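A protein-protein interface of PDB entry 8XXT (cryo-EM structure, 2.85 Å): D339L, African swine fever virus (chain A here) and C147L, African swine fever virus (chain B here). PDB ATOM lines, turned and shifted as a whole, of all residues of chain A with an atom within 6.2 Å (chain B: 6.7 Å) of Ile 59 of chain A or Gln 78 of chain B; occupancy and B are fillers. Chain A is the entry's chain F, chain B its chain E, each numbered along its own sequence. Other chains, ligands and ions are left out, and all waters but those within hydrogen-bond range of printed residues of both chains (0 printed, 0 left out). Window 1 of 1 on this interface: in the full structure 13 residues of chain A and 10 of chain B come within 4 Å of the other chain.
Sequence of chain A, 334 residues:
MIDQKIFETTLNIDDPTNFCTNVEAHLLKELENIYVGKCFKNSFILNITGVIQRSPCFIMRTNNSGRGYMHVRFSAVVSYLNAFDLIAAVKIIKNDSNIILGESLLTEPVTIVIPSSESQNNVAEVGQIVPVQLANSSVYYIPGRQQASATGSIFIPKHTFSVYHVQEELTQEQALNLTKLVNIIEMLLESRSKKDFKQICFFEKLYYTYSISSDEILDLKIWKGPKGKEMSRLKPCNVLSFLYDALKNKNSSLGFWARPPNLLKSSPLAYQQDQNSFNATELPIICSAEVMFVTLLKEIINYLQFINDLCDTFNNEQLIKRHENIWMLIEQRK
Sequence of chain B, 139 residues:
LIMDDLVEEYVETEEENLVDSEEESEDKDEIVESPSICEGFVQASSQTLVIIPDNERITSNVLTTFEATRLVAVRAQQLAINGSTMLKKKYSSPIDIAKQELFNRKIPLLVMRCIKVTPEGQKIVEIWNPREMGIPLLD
The guanidinium group of Arg 70 of chain B sits at hydrogen-bond distance from the backbone carbonyl oxygen of Met 60 of chain A (3.5 Å).
The backbone carbonyl oxygen (O) of Gly 66 of chain A is in hydrogen-bond range of the side-chain amide nitrogen (NE2) of Gln 78 of chain B, 3.4 Å away.
The side-chain amide nitrogen (ND2) of Asn 82 of chain B lies within hydrogen-bond range of the side-chain carboxylate (OD2) of Asp 15 of chain A (2.8 Å).
The guanidinium group (NH1) of Arg 75 of chain B sits at hydrogen-bond distance from the side-chain amide oxygen (OE1) of Gln 78 of chain B, 3.2 Å away.
The backbone carbonyl oxygen (O) of Ser 84 of chain B is in hydrogen-bond range of the guanidinium group (NH2) of Arg 75 of chain B, 2.9 Å away.
OD1 of Asn 82 of chain B sits at hydrogen-bond distance from OG of Ser 84 of chain B, 2.8 Å away.
OD1 of Asp 15 of chain A is in hydrogen-bond range of OG1 of Thr 17 of chain A (2.9 Å).
N of Met 60 of chain A sits at hydrogen-bond distance from O of Arg 67 of chain A (2.7 Å).
The guanidinium group (NH1) of Arg 67 of chain A lies close to the side-chain hydroxyl (OG) of Ser 65 of chain A (3.4 Å).
Among the printed residues, pairs that only touch across the chains: Asp 15 of chain A with Ile 81 of chain B (3.4 Å), Pro 16 of chain A with Gln 78 of chain B (3.4 Å), Thr 17 of chain A with Arg 75 of chain B (3.3 Å), Thr 17 of chain A with Asn 82 of chain B (3.7 Å), Ile 59 of chain A with Arg 70 of chain B (3.9 Å), Ile 59 of chain A with Val 74 of chain B (3.9 Å), Ile 59 of chain A with Gln 78 of chain B (3.3 Å), Arg 61 of chain A with Arg 70 of chain B (3.8 Å), Ser 65 of chain A with Gln 77 of chain B (3.2 Å) and Gly 66 of chain A with Gln 77 of chain B (3.7 Å).
Of chain B, only Arg 70, Val 74 and Gln 78 come within 4 Å of Ile 59 of chain A.
Of the printed residues of chain A, Arg 75 of chain B touches Thr 17.
Of the printed residues of chain A, Asn 82 of chain B touches Asp 15 (2.8 Å) and Thr 17 (3.7 Å).
Thr 62 of chain A touches none of the printed residues of chain B.
The nearest residue of chain B that does not touch Ile 59 of chain A is Leu 109 of chain B (5.2 Å).
The nearest printed residue of chain A that does not touch Gln 77 of chain B is Arg 67 of chain A (5.7 Å).
Of the 15 printed residues of chain B, 7 touch a printed residue of chain A.
Of the 14 printed residues of chain A, 8 touch a printed residue of chain B.
Along chain A the printed residues that touch a printed residue of chain B span positions 15 to 66.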
ATOM      1  N   ASP A  15      14.908  -6.050  10.877  1.00  0.00           N
ATOM      2  CA  ASP A  15      15.934  -6.380   9.888  1.00  0.00           C
ATOM      3  C   ASP A  15      16.862  -5.185   9.741  1.00  0.00           C
ATOM      4  O   ASP A  15      16.727  -4.390   8.803  1.00  0.00           O
ATOM      5  CB  ASP A  15      15.305  -6.759   8.547  1.00  0.00           C
ATOM      6  CG  ASP A  15      16.294  -7.412   7.603  1.00  0.00           C
ATOM      7  OD1 ASP A  15      17.500  -7.436   7.919  1.00  0.00           O
ATOM      8  OD2 ASP A  15      15.864  -7.901   6.540  1.00  0.00           O
ATOM      9  N   PRO A  16      17.817  -5.023  10.659  1.00  0.00           N
ATOM     10  CA  PRO A  16      18.724  -3.867  10.574  1.00  0.00           C
ATOM     11  C   PRO A  16      19.561  -3.834   9.308  1.00  0.00           C
ATOM     12  O   PRO A  16      19.911  -2.745   8.839  1.00  0.00           O
ATOM     13  CB  PRO A  16      19.592  -4.016  11.829  1.00  0.00           C
ATOM     14  CG  PRO A  16      19.481  -5.444  12.209  1.00  0.00           C
ATOM     15  CD  PRO A  16      18.117  -5.885  11.810  1.00  0.00           C
ATOM     16  N   THR A  17      19.902  -4.994   8.743  1.00  0.00           N
ATOM     17  CA  THR A  17      20.684  -5.019   7.511  1.00  0.00           C
ATOM     18  C   THR A  17      19.892  -4.442   6.343  1.00  0.00           C
ATOM     19  O   THR A  17      20.416  -3.647   5.557  1.00  0.00           O
ATOM     20  CB  THR A  17      21.130  -6.447   7.205  1.00  0.00           C
ATOM     21  OG1 THR A  17      20.377  -7.366   8.007  1.00  0.00           O
ATOM     22  CG2 THR A  17      22.605  -6.614   7.509  1.00  0.00           C
ATOM     23  N   CYS A  57      21.732   2.951  14.396  1.00  0.00           N
ATOM     24  CA  CYS A  57      20.899   1.766  14.548  1.00  0.00           C
ATOM     25  C   CYS A  57      21.581   0.767  15.471  1.00  0.00           C
ATOM     26  O   CYS A  57      22.344  -0.089  15.017  1.00  0.00           O
ATOM     27  CB  CYS A  57      20.607   1.129  13.191  1.00  0.00           C
ATOM     28  SG  CYS A  57      19.650  -0.394  13.289  1.00  0.00           S
ATOM     29  N   PHE A  58      21.313   0.877  16.769  1.00  0.00           N
ATOM     30  CA  PHE A  58      21.936   0.008  17.750  1.00  0.00           C
ATOM     31  C   PHE A  58      21.481  -1.434  17.549  1.00  0.00           C
ATOM     32  O   PHE A  58      20.674  -1.742  16.679  1.00  0.00           O
ATOM     33  CB  PHE A  58      21.596   0.464  19.163  1.00  0.00           C
ATOM     34  CG  PHE A  58      22.089   1.837  19.493  1.00  0.00           C
ATOM     35  CD1 PHE A  58      23.433   2.075  19.679  1.00  0.00           C
ATOM     36  CD2 PHE A  58      21.206   2.887  19.628  1.00  0.00           C
ATOM     37  CE1 PHE A  58      23.887   3.332  19.985  1.00  0.00           C
ATOM     38  CE2 PHE A  58      21.656   4.143  19.934  1.00  0.00           C
ATOM     39  CZ  PHE A  58      22.999   4.365  20.112  1.00  0.00           C
ATOM     40  N   ILE A  59      22.026  -2.326  18.370  1.00  0.00           N
ATOM     41  CA  ILE A  59      21.656  -3.735  18.375  1.00  0.00           C
ATOM     42  C   ILE A  59      21.109  -4.074  19.753  1.00  0.00           C
ATOM     43  O   ILE A  59      21.699  -3.695  20.770  1.00  0.00           O
ATOM     44  CB  ILE A  59      22.846  -4.637  18.013  1.00  0.00           C
ATOM     45  CG1 ILE A  59      23.343  -4.330  16.604  1.00  0.00           C
ATOM     46  CG2 ILE A  59      22.455  -6.096  18.114  1.00  0.00           C
ATOM     47  CD1 ILE A  59      22.259  -4.279  15.576  1.00  0.00           C
ATOM     48  N   MET A  60      19.975  -4.770  19.782  1.00  0.00           N
ATOM     49  CA  MET A  60      19.326  -5.112  21.041  1.00  0.00           C
ATOM     50  C   MET A  60      20.262  -5.930  21.918  1.00  0.00           C
ATOM     51  O   MET A  60      20.654  -7.043  21.560  1.00  0.00           O
ATOM     52  CB  MET A  60      18.036  -5.879  20.770  1.00  0.00           C
ATOM     53  CG  MET A  60      16.844  -4.982  20.527  1.00  0.00           C
ATOM     54  SD  MET A  60      15.296  -5.875  20.351  1.00  0.00           S
ATOM     55  CE  MET A  60      14.508  -4.905  19.078  1.00  0.00           C
ATOM     56  N   ARG A  61      20.611  -5.370  23.075  1.00  0.00           N
ATOM     57  CA  ARG A  61      21.619  -5.970  23.938  1.00  0.00           C
ATOM     58  C   ARG A  61      21.058  -7.133  24.748  1.00  0.00           C
ATOM     59  O   ARG A  61      21.660  -8.208  24.798  1.00  0.00           O
ATOM     60  CB  ARG A  61      22.192  -4.902  24.866  1.00  0.00           C
ATOM     61  CG  ARG A  61      23.639  -5.099  25.242  1.00  0.00           C
ATOM     62  CD  ARG A  61      24.096  -3.979  26.157  1.00  0.00           C
ATOM     63  NE  ARG A  61      23.251  -3.881  27.342  1.00  0.00           N
ATOM     64  CZ  ARG A  61      23.461  -4.542  28.471  1.00  0.00           C
ATOM     65  NH1 ARG A  61      24.502  -5.343  28.617  1.00  0.00           N
ATOM     66  NH2 ARG A  61      22.607  -4.394  29.477  1.00  0.00           N
ATOM     67  N   THR A  62      19.899  -6.946  25.374  1.00  0.00           N
ATOM     68  CA  THR A  62      19.395  -7.887  26.364  1.00  0.00           C
ATOM     69  C   THR A  62      18.640  -9.060  25.754  1.00  0.00           C
ATOM     70  O   THR A  62      17.856  -9.705  26.457  1.00  0.00           O
ATOM     71  CB  THR A  62      18.500  -7.166  27.369  1.00  0.00           C
ATOM     72  OG1 THR A  62      17.475  -6.454  26.669  1.00  0.00           O
ATOM     73  CG2 THR A  62      19.312  -6.189  28.192  1.00  0.00           C
ATOM     74  N   SER A  65      18.005 -11.783  19.817  1.00  0.00           N
ATOM     75  CA  SER A  65      17.210 -11.665  18.602  1.00  0.00           C
ATOM     76  C   SER A  65      18.011 -11.070  17.456  1.00  0.00           C
ATOM     77  O   SER A  65      17.707 -11.335  16.289  1.00  0.00           O
ATOM     78  CB  SER A  65      15.967 -10.822  18.869  1.00  0.00           C
ATOM     79  OG  SER A  65      16.324  -9.498  19.216  1.00  0.00           O
ATOM     80  N   GLY A  66      19.021 -10.259  17.760  1.00  0.00           N
ATOM     81  CA  GLY A  66      19.811  -9.620  16.734  1.00  0.00           C
ATOM     82  C   GLY A  66      19.174  -8.402  16.108  1.00  0.00           C
ATOM     83  O   GLY A  66      19.764  -7.818  15.192  1.00  0.00           O
ATOM     84  N   ARG A  67      17.993  -8.006  16.561  1.00  0.00           N
ATOM     85  CA  ARG A  67      17.325  -6.834  16.029  1.00  0.00           C
ATOM     86  C   ARG A  67      17.933  -5.567  16.616  1.00  0.00           C
ATOM     87  O   ARG A  67      18.631  -5.594  17.630  1.00  0.00           O
ATOM     88  CB  ARG A  67      15.828  -6.887  16.334  1.00  0.00           C
ATOM     89  CG  ARG A  67      15.271  -8.291  16.406  1.00  0.00           C
ATOM     90  CD  ARG A  67      13.792  -8.336  16.083  1.00  0.00           C
ATOM     91  NE  ARG A  67      12.999  -7.478  16.952  1.00  0.00           N
ATOM     92  CZ  ARG A  67      12.627  -7.795  18.185  1.00  0.00           C
ATOM     93  NH1 ARG A  67      12.992  -8.937  18.744  1.00  0.00           N
ATOM     94  NH2 ARG A  67      11.864  -6.950  18.871  1.00  0.00           N
ATOM     95  N   GLY A  68      17.667  -4.444  15.953  1.00  0.00           N
ATOM     96  CA  GLY A  68      18.072  -3.146  16.432  1.00  0.00           C
ATOM     97  C   GLY A  68      16.861  -2.308  16.801  1.00  0.00           C
ATOM     98  O   GLY A  68      15.725  -2.635  16.470  1.00  0.00           O
ATOM     99  N   TYR A  69      17.115  -1.215  17.517  1.00  0.00           N
ATOM    100  CA  TYR A  69      16.015  -0.338  17.893  1.00  0.00           C
ATOM    101  C   TYR A  69      16.128   1.051  17.280  1.00  0.00           C
ATOM    102  O   TYR A  69      15.217   1.461  16.555  1.00  0.00           O
ATOM    103  CB  TYR A  69      15.875  -0.249  19.420  1.00  0.00           C
ATOM    104  CG  TYR A  69      17.145  -0.096  20.218  1.00  0.00           C
ATOM    105  CD1 TYR A  69      17.993  -1.171  20.423  1.00  0.00           C
ATOM    106  CD2 TYR A  69      17.465   1.110  20.816  1.00  0.00           C
ATOM    107  CE1 TYR A  69      19.136  -1.037  21.166  1.00  0.00           C
ATOM    108  CE2 TYR A  69      18.604   1.249  21.561  1.00  0.00           C
ATOM    109  CZ  TYR A  69      19.435   0.172  21.734  1.00  0.00           C
ATOM    110  OH  TYR A  69      20.579   0.302  22.477  1.00  0.00           O
ATOM    111  N   ARG B  70      31.245 -10.718  20.047  1.00  0.00           N
ATOM    112  CA  ARG B  70      29.959 -10.043  19.943  1.00  0.00           C
ATOM    113  C   ARG B  70      29.648  -9.664  18.503  1.00  0.00           C
ATOM    114  O   ARG B  70      28.511  -9.822  18.045  1.00  0.00           O
ATOM    115  CB  ARG B  70      29.947  -8.806  20.835  1.00  0.00           C
ATOM    116  CG  ARG B  70      28.701  -7.972  20.701  1.00  0.00           C
ATOM    117  CD  ARG B  70      27.508  -8.654  21.321  1.00  0.00           C
ATOM    118  NE  ARG B  70      26.346  -7.776  21.338  1.00  0.00           N
ATOM    119  CZ  ARG B  70      25.098  -8.191  21.492  1.00  0.00           C
ATOM    120  NH1 ARG B  70      24.813  -9.468  21.672  1.00  0.00           N
ATOM    121  NH2 ARG B  70      24.112  -7.302  21.464  1.00  0.00           N
ATOM    122  N   ALA B  73      28.702 -12.863  16.660  1.00  0.00           N
ATOM    123  CA  ALA B  73      27.394 -13.357  17.077  1.00  0.00           C
ATOM    124  C   ALA B  73      26.272 -12.507  16.499  1.00  0.00           C
ATOM    125  O   ALA B  73      25.270 -13.033  16.000  1.00  0.00           O
ATOM    126  CB  ALA B  73      27.313 -13.391  18.602  1.00  0.00           C
ATOM    127  N   VAL B  74      26.425 -11.183  16.555  1.00  0.00           N
ATOM    128  CA  VAL B  74      25.404 -10.287  16.022  1.00  0.00           C
ATOM    129  C   VAL B  74      25.256 -10.488  14.521  1.00  0.00           C
ATOM    130  O   VAL B  74      24.141 -10.582  13.992  1.00  0.00           O
ATOM    131  CB  VAL B  74      25.743  -8.828  16.365  1.00  0.00           C
ATOM    132  CG1 VAL B  74      24.929  -7.883  15.514  1.00  0.00           C
ATOM    133  CG2 VAL B  74      25.501  -8.565  17.833  1.00  0.00           C
ATOM    134  N   ARG B  75      26.383 -10.565  13.810  1.00  0.00           N
ATOM    135  CA  ARG B  75      26.326 -10.758  12.368  1.00  0.00           C
ATOM    136  C   ARG B  75      25.717 -12.105  12.015  1.00  0.00           C
ATOM    137  O   ARG B  75      24.960 -12.215  11.048  1.00  0.00           O
ATOM    138  CB  ARG B  75      27.718 -10.625  11.765  1.00  0.00           C
ATOM    139  CG  ARG B  75      27.751 -10.853  10.274  1.00  0.00           C
ATOM    140  CD  ARG B  75      27.470  -9.571   9.529  1.00  0.00           C
ATOM    141  NE  ARG B  75      26.753  -9.807   8.283  1.00  0.00           N
ATOM    142  CZ  ARG B  75      25.535  -9.352   8.025  1.00  0.00           C
ATOM    143  NH1 ARG B  75      24.877  -8.609   8.898  1.00  0.00           N
ATOM    144  NH2 ARG B  75      24.967  -9.646   6.860  1.00  0.00           N
ATOM    145  N   ALA B  76      26.037 -13.147  12.783  1.00  0.00           N
ATOM    146  CA  ALA B  76      25.479 -14.465  12.512  1.00  0.00           C
ATOM    147  C   ALA B  76      23.976 -14.488  12.749  1.00  0.00           C
ATOM    148  O   ALA B  76      23.233 -15.104  11.981  1.00  0.00           O
ATOM    149  CB  ALA B  76      26.182 -15.511  13.371  1.00  0.00           C
ATOM    150  N   GLN B  77      23.503 -13.815  13.797  1.00  0.00           N
ATOM    151  CA  GLN B  77      22.062 -13.741  14.011  1.00  0.00           C
ATOM    152  C   GLN B  77      21.377 -12.969  12.890  1.00  0.00           C
ATOM    153  O   GLN B  77      20.312 -13.373  12.403  1.00  0.00           O
ATOM    154  CB  GLN B  77      21.757 -13.101  15.362  1.00  0.00           C
ATOM    155  CG  GLN B  77      20.287 -13.121  15.707  1.00  0.00           C
ATOM    156  CD  GLN B  77      19.715 -14.519  15.709  1.00  0.00           C
ATOM    157  OE1 GLN B  77      20.160 -15.384  16.461  1.00  0.00           O
ATOM    158  NE2 GLN B  77      18.727 -14.753  14.858  1.00  0.00           N
ATOM    159  N   GLN B  78      21.979 -11.861  12.457  1.00  0.00           N
ATOM    160  CA  GLN B  78      21.375 -11.090  11.377  1.00  0.00           C
ATOM    161  C   GLN B  78      21.416 -11.845  10.057  1.00  0.00           C
ATOM    162  O   GLN B  78      20.542 -11.650   9.209  1.00  0.00           O
ATOM    163  CB  GLN B  78      22.065  -9.739  11.248  1.00  0.00           C
ATOM    164  CG  GLN B  78      21.789  -8.825  12.418  1.00  0.00           C
ATOM    165  CD  GLN B  78      22.582  -7.552  12.352  1.00  0.00           C
ATOM    166  OE1 GLN B  78      23.352  -7.336  11.420  1.00  0.00           O
ATOM    167  NE2 GLN B  78      22.398  -6.693  13.339  1.00  0.00           N
ATOM    168  N   LEU B  79      22.417 -12.704   9.865  1.00  0.00           N
ATOM    169  CA  LEU B  79      22.426 -13.600   8.718  1.00  0.00           C
ATOM    170  C   LEU B  79      21.435 -14.735   8.883  1.00  0.00           C
ATOM    171  O   LEU B  79      21.065 -15.372   7.894  1.00  0.00           O
ATOM    172  CB  LEU B  79      23.824 -14.173   8.509  1.00  0.00           C
ATOM    173  CG  LEU B  79      24.876 -13.231   7.942  1.00  0.00           C
ATOM    174  CD1 LEU B  79      26.245 -13.807   8.206  1.00  0.00           C
ATOM    175  CD2 LEU B  79      24.655 -13.017   6.463  1.00  0.00           C
ATOM    176  N   ALA B  80      21.038 -15.032  10.117  1.00  0.00           N
ATOM    177  CA  ALA B  80      19.964 -15.992  10.332  1.00  0.00           C
ATOM    178  C   ALA B  80      18.609 -15.389   9.995  1.00  0.00           C
ATOM    179  O   ALA B  80      17.711 -16.106   9.540  1.00  0.00           O
ATOM    180  CB  ALA B  80      19.983 -16.490  11.774  1.00  0.00           C
ATOM    181  N   ILE B  81      18.435 -14.087  10.207  1.00  0.00           N
ATOM    182  CA  ILE B  81      17.173 -13.453   9.831  1.00  0.00           C
ATOM    183  C   ILE B  81      17.207 -12.945   8.389  1.00  0.00           C
ATOM    184  O   ILE B  81      16.235 -13.111   7.650  1.00  0.00           O
ATOM    185  CB  ILE B  81      16.807 -12.331  10.830  1.00  0.00           C
ATOM    186  CG1 ILE B  81      17.823 -11.191  10.806  1.00  0.00           C
ATOM    187  CG2 ILE B  81      16.692 -12.895  12.234  1.00  0.00           C
ATOM    188  CD1 ILE B  81      17.308  -9.933  10.153  1.00  0.00           C
ATOM    189  N   ASN B  82      18.304 -12.328   7.962  1.00  0.00           N
ATOM    190  CA  ASN B  82      18.484 -11.914   6.578  1.00  0.00           C
ATOM    191  C   ASN B  82      19.252 -13.005   5.829  1.00  0.00           C
ATOM    192  O   ASN B  82      19.370 -14.137   6.297  1.00  0.00           O
ATOM    193  CB  ASN B  82      19.188 -10.562   6.516  1.00  0.00           C
ATOM    194  CG  ASN B  82      18.975  -9.851   5.197  1.00  0.00           C
ATOM    195  OD1 ASN B  82      19.747 -10.024   4.257  1.00  0.00           O
ATOM    196  ND2 ASN B  82      17.923  -9.047   5.120  1.00  0.00           N
ATOM    197  N   GLY B  83      19.755 -12.688   4.639  1.00  0.00           N
ATOM    198  CA  GLY B  83      20.591 -13.628   3.918  1.00  0.00           C
ATOM    199  C   GLY B  83      21.684 -12.986   3.089  1.00  0.00           C
ATOM    200  O   GLY B  83      22.409 -13.678   2.370  1.00  0.00           O
ATOM    201  N   SER B  84      21.827 -11.668   3.192  1.00  0.00           N
ATOM    202  CA  SER B  84      22.752 -10.925   2.350  1.00  0.00           C
ATOM    203  C   SER B  84      24.139 -10.879   2.977  1.00  0.00           C
ATOM    204  O   SER B  84      24.285 -10.643   4.178  1.00  0.00           O
ATOM    205  CB  SER B  84      22.244  -9.502   2.121  1.00  0.00           C
ATOM    206  OG  SER B  84      22.131  -8.803   3.347  1.00  0.00           O
ATOM    207  N   PRO B 108      29.485  -5.607   8.262  1.00  0.00           N
ATOM    208  CA  PRO B 108      28.762  -4.331   8.215  1.00  0.00           C
ATOM    209  C   PRO B 108      28.345  -3.822   9.584  1.00  0.00           C
ATOM    210  O   PRO B 108      27.231  -3.320   9.747  1.00  0.00           O
ATOM    211  CB  PRO B 108      27.537  -4.670   7.362  1.00  0.00           C
ATOM    212  CG  PRO B 108      27.273  -6.087   7.698  1.00  0.00           C
ATOM    213  CD  PRO B 108      28.619  -6.736   7.892  1.00  0.00           C
ATOM    214  N   LEU B 109      29.230  -3.927  10.566  1.00  0.00           N
ATOM    215  CA  LEU B 109      28.920  -3.547  11.933  1.00  0.00           C
ATOM    216  C   LEU B 109      30.001  -2.612  12.442  1.00  0.00           C
ATOM    217  O   LEU B 109      31.152  -2.683  12.012  1.00  0.00           O
ATOM    218  CB  LEU B 109      28.825  -4.772  12.852  1.00  0.00           C
ATOM    219  CG  LEU B 109      27.829  -5.868  12.476  1.00  0.00           C
ATOM    220  CD1 LEU B 109      27.972  -7.049  13.401  1.00  0.00           C
ATOM    221  CD2 LEU B 109      26.419  -5.337  12.521  1.00  0.00           C
